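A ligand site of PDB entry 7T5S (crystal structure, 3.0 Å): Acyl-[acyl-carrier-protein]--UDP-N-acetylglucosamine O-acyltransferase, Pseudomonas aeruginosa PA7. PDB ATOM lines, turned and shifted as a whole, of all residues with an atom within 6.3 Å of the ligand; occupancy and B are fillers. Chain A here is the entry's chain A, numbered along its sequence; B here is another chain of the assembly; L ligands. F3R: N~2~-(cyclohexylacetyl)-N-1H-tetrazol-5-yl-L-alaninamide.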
ATOM      1  N   VAL A 132     -11.685   4.062 -13.481  1.00  0.00           N
ATOM      2  CA  VAL A 132     -12.085   2.618 -13.465  1.00  0.00           C
ATOM      3  C   VAL A 132     -13.469   2.505 -12.812  1.00  0.00           C
ATOM      4  O   VAL A 132     -13.845   3.422 -12.063  1.00  0.00           O
ATOM      5  CB  VAL A 132     -11.035   1.757 -12.754  1.00  0.00           C
ATOM      6  CG1 VAL A 132     -11.467   0.301 -12.655  1.00  0.00           C
ATOM      7  CG2 VAL A 132      -9.662   1.845 -13.427  1.00  0.00           C
ATOM      8  N   ASN A 133     -14.174   1.413 -13.121  1.00  0.00           N
ATOM      9  CA  ASN A 133     -15.552   1.097 -12.644  1.00  0.00           C
ATOM     10  C   ASN A 133     -15.813   1.701 -11.269  1.00  0.00           C
ATOM     11  O   ASN A 133     -15.087   1.355 -10.320  1.00  0.00           O
ATOM     12  CB  ASN A 133     -15.792  -0.412 -12.597  1.00  0.00           C
ATOM     13  CG  ASN A 133     -15.383  -1.124 -13.874  1.00  0.00           C
ATOM     14  OD1 ASN A 133     -14.265  -0.946 -14.363  1.00  0.00           O
ATOM     15  ND2 ASN A 133     -16.263  -1.945 -14.425  1.00  0.00           N
ATOM     16  N   ILE A 148      -4.722   7.908 -13.488  1.00  0.00           N
ATOM     17  CA  ILE A 148      -5.447   6.605 -13.445  1.00  0.00           C
ATOM     18  C   ILE A 148      -6.016   6.402 -12.042  1.00  0.00           C
ATOM     19  O   ILE A 148      -5.221   6.243 -11.106  1.00  0.00           O
ATOM     20  CB  ILE A 148      -4.531   5.441 -13.874  1.00  0.00           C
ATOM     21  CG1 ILE A 148      -4.021   5.633 -15.308  1.00  0.00           C
ATOM     22  CG2 ILE A 148      -5.226   4.111 -13.693  1.00  0.00           C
ATOM     23  CD1 ILE A 148      -2.968   4.651 -15.749  1.00  0.00           C
ATOM     24  N   LEU A 149      -7.339   6.413 -11.909  1.00  0.00           N
ATOM     25  CA  LEU A 149      -8.065   6.139 -10.640  1.00  0.00           C
ATOM     26  C   LEU A 149      -8.623   4.709 -10.670  1.00  0.00           C
ATOM     27  O   LEU A 149      -9.576   4.468 -11.436  1.00  0.00           O
ATOM     28  CB  LEU A 149      -9.170   7.180 -10.457  1.00  0.00           C
ATOM     29  CG  LEU A 149      -8.704   8.633 -10.437  1.00  0.00           C
ATOM     30  CD1 LEU A 149      -9.868   9.572 -10.205  1.00  0.00           C
ATOM     31  CD2 LEU A 149      -7.650   8.856  -9.362  1.00  0.00           C
ATOM     32  N   SER A 150      -8.020   3.807  -9.878  1.00  0.00           N
ATOM     33  CA  SER A 150      -8.380   2.370  -9.795  1.00  0.00           C
ATOM     34  C   SER A 150      -9.849   2.228  -9.393  1.00  0.00           C
ATOM     35  O   SER A 150     -10.456   3.238  -8.967  1.00  0.00           O
ATOM     36  CB  SER A 150      -7.496   1.635  -8.818  1.00  0.00           C
ATOM     37  OG  SER A 150      -6.151   1.616  -9.267  1.00  0.00           O
ATOM     38  N   GLY A 151     -10.385   1.013  -9.514  1.00  0.00           N
ATOM     39  CA  GLY A 151     -11.804   0.686  -9.274  1.00  0.00           C
ATOM     40  C   GLY A 151     -12.287   1.224  -7.941  1.00  0.00           C
ATOM     41  O   GLY A 151     -11.638   0.931  -6.914  1.00  0.00           O
ATOM     42  N   TYR A 152     -13.383   1.986  -7.974  1.00  0.00           N
ATOM     43  CA  TYR A 152     -14.138   2.449  -6.779  1.00  0.00           C
ATOM     44  C   TYR A 152     -13.307   3.450  -5.952  1.00  0.00           C
ATOM     45  O   TYR A 152     -13.419   3.441  -4.711  1.00  0.00           O
ATOM     46  CB  TYR A 152     -14.579   1.257  -5.922  1.00  0.00           C
ATOM     47  CG  TYR A 152     -15.648   0.377  -6.531  1.00  0.00           C
ATOM     48  CD1 TYR A 152     -15.414  -0.333  -7.683  1.00  0.00           C
ATOM     49  CD2 TYR A 152     -16.872   0.223  -5.901  1.00  0.00           C
ATOM     50  CE1 TYR A 152     -16.390  -1.154  -8.227  1.00  0.00           C
ATOM     51  CE2 TYR A 152     -17.857  -0.599  -6.428  1.00  0.00           C
ATOM     52  CZ  TYR A 152     -17.612  -1.298  -7.595  1.00  0.00           C
ATOM     53  OH  TYR A 152     -18.580  -2.104  -8.122  1.00  0.00           O
ATOM     54  N   PHE A 166      -1.702   7.841  -9.689  1.00  0.00           N
ATOM     55  CA  PHE A 166      -2.385   6.519  -9.649  1.00  0.00           C
ATOM     56  C   PHE A 166      -2.956   6.306  -8.248  1.00  0.00           C
ATOM     57  O   PHE A 166      -2.205   6.439  -7.259  1.00  0.00           O
ATOM     58  CB  PHE A 166      -1.400   5.409 -10.014  1.00  0.00           C
ATOM     59  CG  PHE A 166      -1.942   4.013  -9.886  1.00  0.00           C
ATOM     60  CD1 PHE A 166      -2.629   3.415 -10.924  1.00  0.00           C
ATOM     61  CD2 PHE A 166      -1.733   3.279  -8.736  1.00  0.00           C
ATOM     62  CE1 PHE A 166      -3.112   2.123 -10.800  1.00  0.00           C
ATOM     63  CE2 PHE A 166      -2.219   1.986  -8.603  1.00  0.00           C
ATOM     64  CZ  PHE A 166      -2.911   1.409  -9.641  1.00  0.00           C
ATOM     65  N   SER A 167      -4.258   6.007  -8.160  1.00  0.00           N
ATOM     66  CA  SER A 167      -4.940   5.582  -6.917  1.00  0.00           C
ATOM     67  C   SER A 167      -5.156   4.064  -6.950  1.00  0.00           C
ATOM     68  O   SER A 167      -5.565   3.565  -8.015  1.00  0.00           O
ATOM     69  CB  SER A 167      -6.246   6.320  -6.723  1.00  0.00           C
ATOM     70  OG  SER A 167      -7.231   5.832  -7.620  1.00  0.00           O
ATOM     71  N   GLY A 168      -4.851   3.371  -5.849  1.00  0.00           N
ATOM     72  CA  GLY A 168      -5.178   1.944  -5.658  1.00  0.00           C
ATOM     73  C   GLY A 168      -6.683   1.743  -5.562  1.00  0.00           C
ATOM     74  O   GLY A 168      -7.391   2.729  -5.305  1.00  0.00           O
ATOM     75  N   MET A 169      -7.155   0.513  -5.776  1.00  0.00           N
ATOM     76  CA  MET A 169      -8.612   0.193  -5.815  1.00  0.00           C
ATOM     77  C   MET A 169      -9.209   0.376  -4.420  1.00  0.00           C
ATOM     78  O   MET A 169      -8.539   0.001  -3.424  1.00  0.00           O
ATOM     79  CB  MET A 169      -8.865  -1.230  -6.332  1.00  0.00           C
ATOM     80  CG  MET A 169      -8.333  -2.337  -5.439  1.00  0.00           C
ATOM     81  SD  MET A 169      -8.526  -3.980  -6.208  1.00  0.00           S
ATOM     82  CE  MET A 169      -7.188  -4.853  -5.405  1.00  0.00           C
ATOM     83  N   GLY A 170     -10.419   0.943  -4.352  1.00  0.00           N
ATOM     84  CA  GLY A 170     -11.166   1.216  -3.115  1.00  0.00           C
ATOM     85  C   GLY A 170     -10.500   2.294  -2.275  1.00  0.00           C
ATOM     86  O   GLY A 170     -10.698   2.273  -1.034  1.00  0.00           O
ATOM     87  N   PHE A 184      -3.023   4.794  -2.000  1.00  0.00           N
ATOM     88  CA  PHE A 184      -3.695   3.496  -1.703  1.00  0.00           C
ATOM     89  C   PHE A 184      -4.478   3.593  -0.390  1.00  0.00           C
ATOM     90  O   PHE A 184      -3.958   4.173   0.572  1.00  0.00           O
ATOM     91  CB  PHE A 184      -2.679   2.367  -1.590  1.00  0.00           C
ATOM     92  CG  PHE A 184      -1.906   2.072  -2.850  1.00  0.00           C
ATOM     93  CD1 PHE A 184      -0.746   2.786  -3.149  1.00  0.00           C
ATOM     94  CD2 PHE A 184      -2.310   1.081  -3.738  1.00  0.00           C
ATOM     95  CE1 PHE A 184      -0.032   2.524  -4.311  1.00  0.00           C
ATOM     96  CE2 PHE A 184      -1.586   0.826  -4.894  1.00  0.00           C
ATOM     97  CZ  PHE A 184      -0.452   1.545  -5.184  1.00  0.00           C
ATOM     98  N   HIS B 118     -20.014  -6.496 -11.343  1.00  0.00           N
ATOM     99  CA  HIS B 118     -19.231  -6.457 -12.608  1.00  0.00           C
ATOM    100  C   HIS B 118     -18.395  -7.729 -12.751  1.00  0.00           C
ATOM    101  O   HIS B 118     -17.742  -8.139 -11.767  1.00  0.00           O
ATOM    102  CB  HIS B 118     -18.359  -5.194 -12.670  1.00  0.00           C
ATOM    103  CG  HIS B 118     -17.456  -5.159 -13.850  1.00  0.00           C
ATOM    104  ND1 HIS B 118     -17.931  -5.068 -15.137  1.00  0.00           N
ATOM    105  CD2 HIS B 118     -16.109  -5.192 -13.951  1.00  0.00           C
ATOM    106  CE1 HIS B 118     -16.915  -5.040 -15.977  1.00  0.00           C
ATOM    107  NE2 HIS B 118     -15.794  -5.125 -15.284  1.00  0.00           N
ATOM    108  N   ALA B 136     -17.096  -6.399  -7.987  1.00  0.00           N
ATOM    109  CA  ALA B 136     -16.376  -6.108  -9.235  1.00  0.00           C
ATOM    110  C   ALA B 136     -15.189  -7.056  -9.400  1.00  0.00           C
ATOM    111  O   ALA B 136     -14.262  -6.980  -8.575  1.00  0.00           O
ATOM    112  CB  ALA B 136     -15.952  -4.663  -9.227  1.00  0.00           C
ATOM    113  N   LEU B 137     -15.234  -7.922 -10.418  1.00  0.00           N
ATOM    114  CA  LEU B 137     -14.131  -8.826 -10.836  1.00  0.00           C
ATOM    115  C   LEU B 137     -13.434  -8.211 -12.051  1.00  0.00           C
ATOM    116  O   LEU B 137     -14.118  -7.957 -13.055  1.00  0.00           O
ATOM    117  CB  LEU B 137     -14.688 -10.218 -11.133  1.00  0.00           C
ATOM    118  CG  LEU B 137     -15.682 -10.785 -10.112  1.00  0.00           C
ATOM    119  CD1 LEU B 137     -16.056 -12.218 -10.455  1.00  0.00           C
ATOM    120  CD2 LEU B 137     -15.143 -10.709  -8.696  1.00  0.00           C
ATOM    121  N   ALA B 138     -12.119  -7.979 -11.947  1.00  0.00           N
ATOM    122  CA  ALA B 138     -11.311  -7.148 -12.879  1.00  0.00           C
ATOM    123  C   ALA B 138     -11.266  -7.771 -14.277  1.00  0.00           C
ATOM    124  O   ALA B 138     -11.784  -7.148 -15.224  1.00  0.00           O
ATOM    125  CB  ALA B 138      -9.927  -6.945 -12.336  1.00  0.00           C
ATOM    126  N   GLY B 139     -10.625  -8.931 -14.395  1.00  0.00           N
ATOM    127  CA  GLY B 139     -10.395  -9.623 -15.671  1.00  0.00           C
ATOM    128  C   GLY B 139      -9.422 -10.770 -15.481  1.00  0.00           C
ATOM    129  O   GLY B 139      -8.435 -10.581 -14.750  1.00  0.00           O
ATOM    130  N   THR B 153     -17.230  -6.033  -2.797  1.00  0.00           N
ATOM    131  CA  THR B 153     -15.931  -6.760  -2.847  1.00  0.00           C
ATOM    132  C   THR B 153     -15.259  -6.468  -4.188  1.00  0.00           C
ATOM    133  O   THR B 153     -15.950  -6.553  -5.220  1.00  0.00           O
ATOM    134  CB  THR B 153     -16.094  -8.273  -2.626  1.00  0.00           C
ATOM    135  OG1 THR B 153     -16.714  -8.486  -1.364  1.00  0.00           O
ATOM    136  CG2 THR B 153     -14.773  -9.005  -2.677  1.00  0.00           C
ATOM    137  N   LEU B 154     -13.968  -6.131  -4.154  1.00  0.00           N
ATOM    138  CA  LEU B 154     -13.146  -5.820  -5.358  1.00  0.00           C
ATOM    139  C   LEU B 154     -12.112  -6.940  -5.541  1.00  0.00           C
ATOM    140  O   LEU B 154     -11.600  -7.450  -4.528  1.00  0.00           O
ATOM    141  CB  LEU B 154     -12.463  -4.467  -5.158  1.00  0.00           C
ATOM    142  CG  LEU B 154     -13.395  -3.301  -4.816  1.00  0.00           C
ATOM    143  CD1 LEU B 154     -12.599  -2.018  -4.611  1.00  0.00           C
ATOM    144  CD2 LEU B 154     -14.464  -3.122  -5.891  1.00  0.00           C
ATOM    145  N   VAL B 155     -11.816  -7.296  -6.793  1.00  0.00           N
ATOM    146  CA  VAL B 155     -10.911  -8.417  -7.167  1.00  0.00           C
ATOM    147  C   VAL B 155     -10.011  -7.986  -8.330  1.00  0.00           C
ATOM    148  O   VAL B 155     -10.562  -7.724  -9.412  1.00  0.00           O
ATOM    149  CB  VAL B 155     -11.713  -9.692  -7.499  1.00  0.00           C
ATOM    150  CG1 VAL B 155     -10.822 -10.921  -7.609  1.00  0.00           C
ATOM    151  CG2 VAL B 155     -12.819  -9.939  -6.479  1.00  0.00           C
ATOM    152  N   HIS B 156      -8.695  -7.932  -8.087  1.00  0.00           N
ATOM    153  CA  HIS B 156      -7.612  -7.548  -9.036  1.00  0.00           C
ATOM    154  C   HIS B 156      -7.571  -8.524 -10.213  1.00  0.00           C
ATOM    155  O   HIS B 156      -8.155  -9.636 -10.088  1.00  0.00           O
ATOM    156  CB  HIS B 156      -6.273  -7.505  -8.296  1.00  0.00           C
ATOM    157  CG  HIS B 156      -5.158  -6.821  -9.028  1.00  0.00           C
ATOM    158  ND1 HIS B 156      -4.323  -7.475  -9.920  1.00  0.00           N
ATOM    159  CD2 HIS B 156      -4.710  -5.540  -8.968  1.00  0.00           C
ATOM    160  CE1 HIS B 156      -3.442  -6.613 -10.404  1.00  0.00           C
ATOM    161  NE2 HIS B 156      -3.650  -5.435  -9.823  1.00  0.00           N
ATOM    162  N   GLN B 157      -6.912  -8.136 -11.313  1.00  0.00           N
ATOM    163  CA  GLN B 157      -6.639  -8.993 -12.505  1.00  0.00           C
ATOM    164  C   GLN B 157      -5.948 -10.300 -12.059  1.00  0.00           C
ATOM    165  O   GLN B 157      -5.056 -10.227 -11.185  1.00  0.00           O
ATOM    166  CB  GLN B 157      -5.732  -8.266 -13.498  1.00  0.00           C
ATOM    167  CG  GLN B 157      -6.456  -7.732 -14.730  1.00  0.00           C
ATOM    168  CD  GLN B 157      -5.481  -7.305 -15.810  1.00  0.00           C
ATOM    169  OE1 GLN B 157      -4.339  -6.925 -15.532  1.00  0.00           O
ATOM    170  NE2 GLN B 157      -5.923  -7.376 -17.063  1.00  0.00           N
ATOM    171  N   ILE B 173      -9.312  -7.491  -2.878  1.00  0.00           N
ATOM    172  CA  ILE B 173      -8.484  -8.715  -3.043  1.00  0.00           C
ATOM    173  C   ILE B 173      -7.461  -8.479  -4.163  1.00  0.00           C
ATOM    174  O   ILE B 173      -7.880  -8.355  -5.326  1.00  0.00           O
ATOM    175  CB  ILE B 173      -9.385  -9.927  -3.318  1.00  0.00           C
ATOM    176  CG1 ILE B 173     -10.410 -10.131  -2.195  1.00  0.00           C
ATOM    177  CG2 ILE B 173      -8.560 -11.174  -3.565  1.00  0.00           C
ATOM    178  CD1 ILE B 173     -11.471 -11.152  -2.510  1.00  0.00           C
ATOM    179  N   ARG B 254      -0.307 -15.088  -8.375  1.00  0.00           N
ATOM    180  CA  ARG B 254      -0.078 -13.739  -7.788  1.00  0.00           C
ATOM    181  C   ARG B 254       0.405 -13.856  -6.342  1.00  0.00           C
ATOM    182  O   ARG B 254       0.832 -12.805  -5.797  1.00  0.00           O
ATOM    183  CB  ARG B 254      -1.377 -12.916  -7.840  1.00  0.00           C
ATOM    184  CG  ARG B 254      -1.781 -12.491  -9.236  1.00  0.00           C
ATOM    185  CD  ARG B 254      -2.788 -11.352  -9.263  1.00  0.00           C
ATOM    186  NE  ARG B 254      -2.447 -10.256  -8.362  1.00  0.00           N
ATOM    187  CZ  ARG B 254      -1.555  -9.293  -8.604  1.00  0.00           C
ATOM    188  NH1 ARG B 254      -0.873  -9.269  -9.741  1.00  0.00           N
ATOM    189  NH2 ARG B 254      -1.343  -8.345  -7.706  1.00  0.00           N
HETATM  190  C15 F3R L   1     -10.226  -4.174 -10.381  1.00  0.00           C
HETATM  191  C17 F3R L   1     -11.838  -3.068  -8.690  1.00  0.00           C
HETATM  192  C20 F3R L   1     -11.343  -3.980 -11.468  1.00  0.00           C
HETATM  193  C01 F3R L   1      -6.023  -0.135 -12.662  1.00  0.00           C
HETATM  194  C02 F3R L   1      -6.708  -1.387 -12.039  1.00  0.00           C
HETATM  195  C03 F3R L   1      -5.843  -1.839 -10.803  1.00  0.00           C
HETATM  196  O04 F3R L   1      -5.345  -2.981 -10.948  1.00  0.00           O
HETATM  197  N05 F3R L   1      -5.629  -1.119  -9.635  1.00  0.00           N
HETATM  198  C06 F3R L   1      -4.855  -1.598  -8.517  1.00  0.00           C
HETATM  199  N07 F3R L   1      -5.153  -1.361  -7.200  1.00  0.00           N
HETATM  200  N08 F3R L   1      -4.219  -1.984  -6.444  1.00  0.00           N
HETATM  201  N09 F3R L   1      -3.314  -2.634  -7.334  1.00  0.00           N
HETATM  202  N10 F3R L   1      -3.724  -2.393  -8.605  1.00  0.00           N
HETATM  203  N11 F3R L   1      -8.089  -0.992 -11.591  1.00  0.00           N
HETATM  204  C12 F3R L   1      -9.043  -1.863 -10.987  1.00  0.00           C
HETATM  205  O13 F3R L   1     -10.132  -1.380 -10.673  1.00  0.00           O
HETATM  206  C14 F3R L   1      -8.897  -3.363 -10.673  1.00  0.00           C
HETATM  207  C16 F3R L   1     -10.731  -4.082  -8.903  1.00  0.00           C
HETATM  208  C18 F3R L   1     -12.988  -3.306  -9.647  1.00  0.00           C
HETATM  209  C19 F3R L   1     -12.546  -3.109 -11.081  1.00  0.00           C
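Residues that only touch the ligand: Val 132 (2.9 Å), Phe 166 (3.7 Å), Gly 168 (3.6 Å), Ala 136 of chain B (3.3 Å), Ala 138 of chain B (3.4 Å), Leu 154 of chain B (3.8 Å) and Val 155 of chain B (3.7 Å).
Hydrophobic or aromatic side chains within 4 Å of the ligand: Val 132, Phe 166, Met 169, Ala 136 of chain B, Ala 138 of chain B, Leu 154 of chain B and His 156 of chain B.
The nearest printed residue that does not touch the ligand is Phe 184 (4.2 Å).
An oxygen (O13) of the ligand is in hydrogen-bond range of the backbone NH (N) of Gly 151 (2.7 Å).
A nitrogen (N05) of the ligand lies within hydrogen-bond range of the side-chain hydroxyl (OG) of Ser 150 (2.8 Å).
The backbone NH of Met 169 lies within hydrogen-bond range of a nitrogen (N07) of the ligand, 3.1 Å away.
A ring nitrogen (NE2) of His 156 of chain B lies within hydrogen-bond range of an oxygen (O04) of the ligand (3.2 Å).
The backbone carbonyl oxygen (O) of Thr 153 of chain B is in hydrogen-bond range of the backbone NH (N) of Ala 136 of chain B (3.0 Å).
The backbone NH of Ser 150 lies close to the backbone carbonyl oxygen of Ser 167, 3.1 Å away.
The backbone NH (N) of Ala 138 of chain B sits at hydrogen-bond distance from the backbone carbonyl oxygen (O) of Val 155 of chain B (3.0 Å).
N of Val 155 of chain B lies within hydrogen-bond range of O of Ala 136 of chain B.
The backbone carbonyl oxygen of Leu 154 of chain B is in hydrogen-bond range of the backbone NH of Ile 173 of chain B (2.8 Å).
The backbone NH of His 156 of chain B lies within hydrogen-bond range of the backbone carbonyl oxygen of Ile 173 of chain B (2.9 Å).
The backbone carbonyl oxygen (O) of Gly 151 sits at hydrogen-bond distance from the backbone NH (N) of Gly 170 (2.8 Å).
The backbone carbonyl oxygen (O) of Leu 149 lies within hydrogen-bond range of the backbone NH (N) of Val 132 (3.0 Å).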
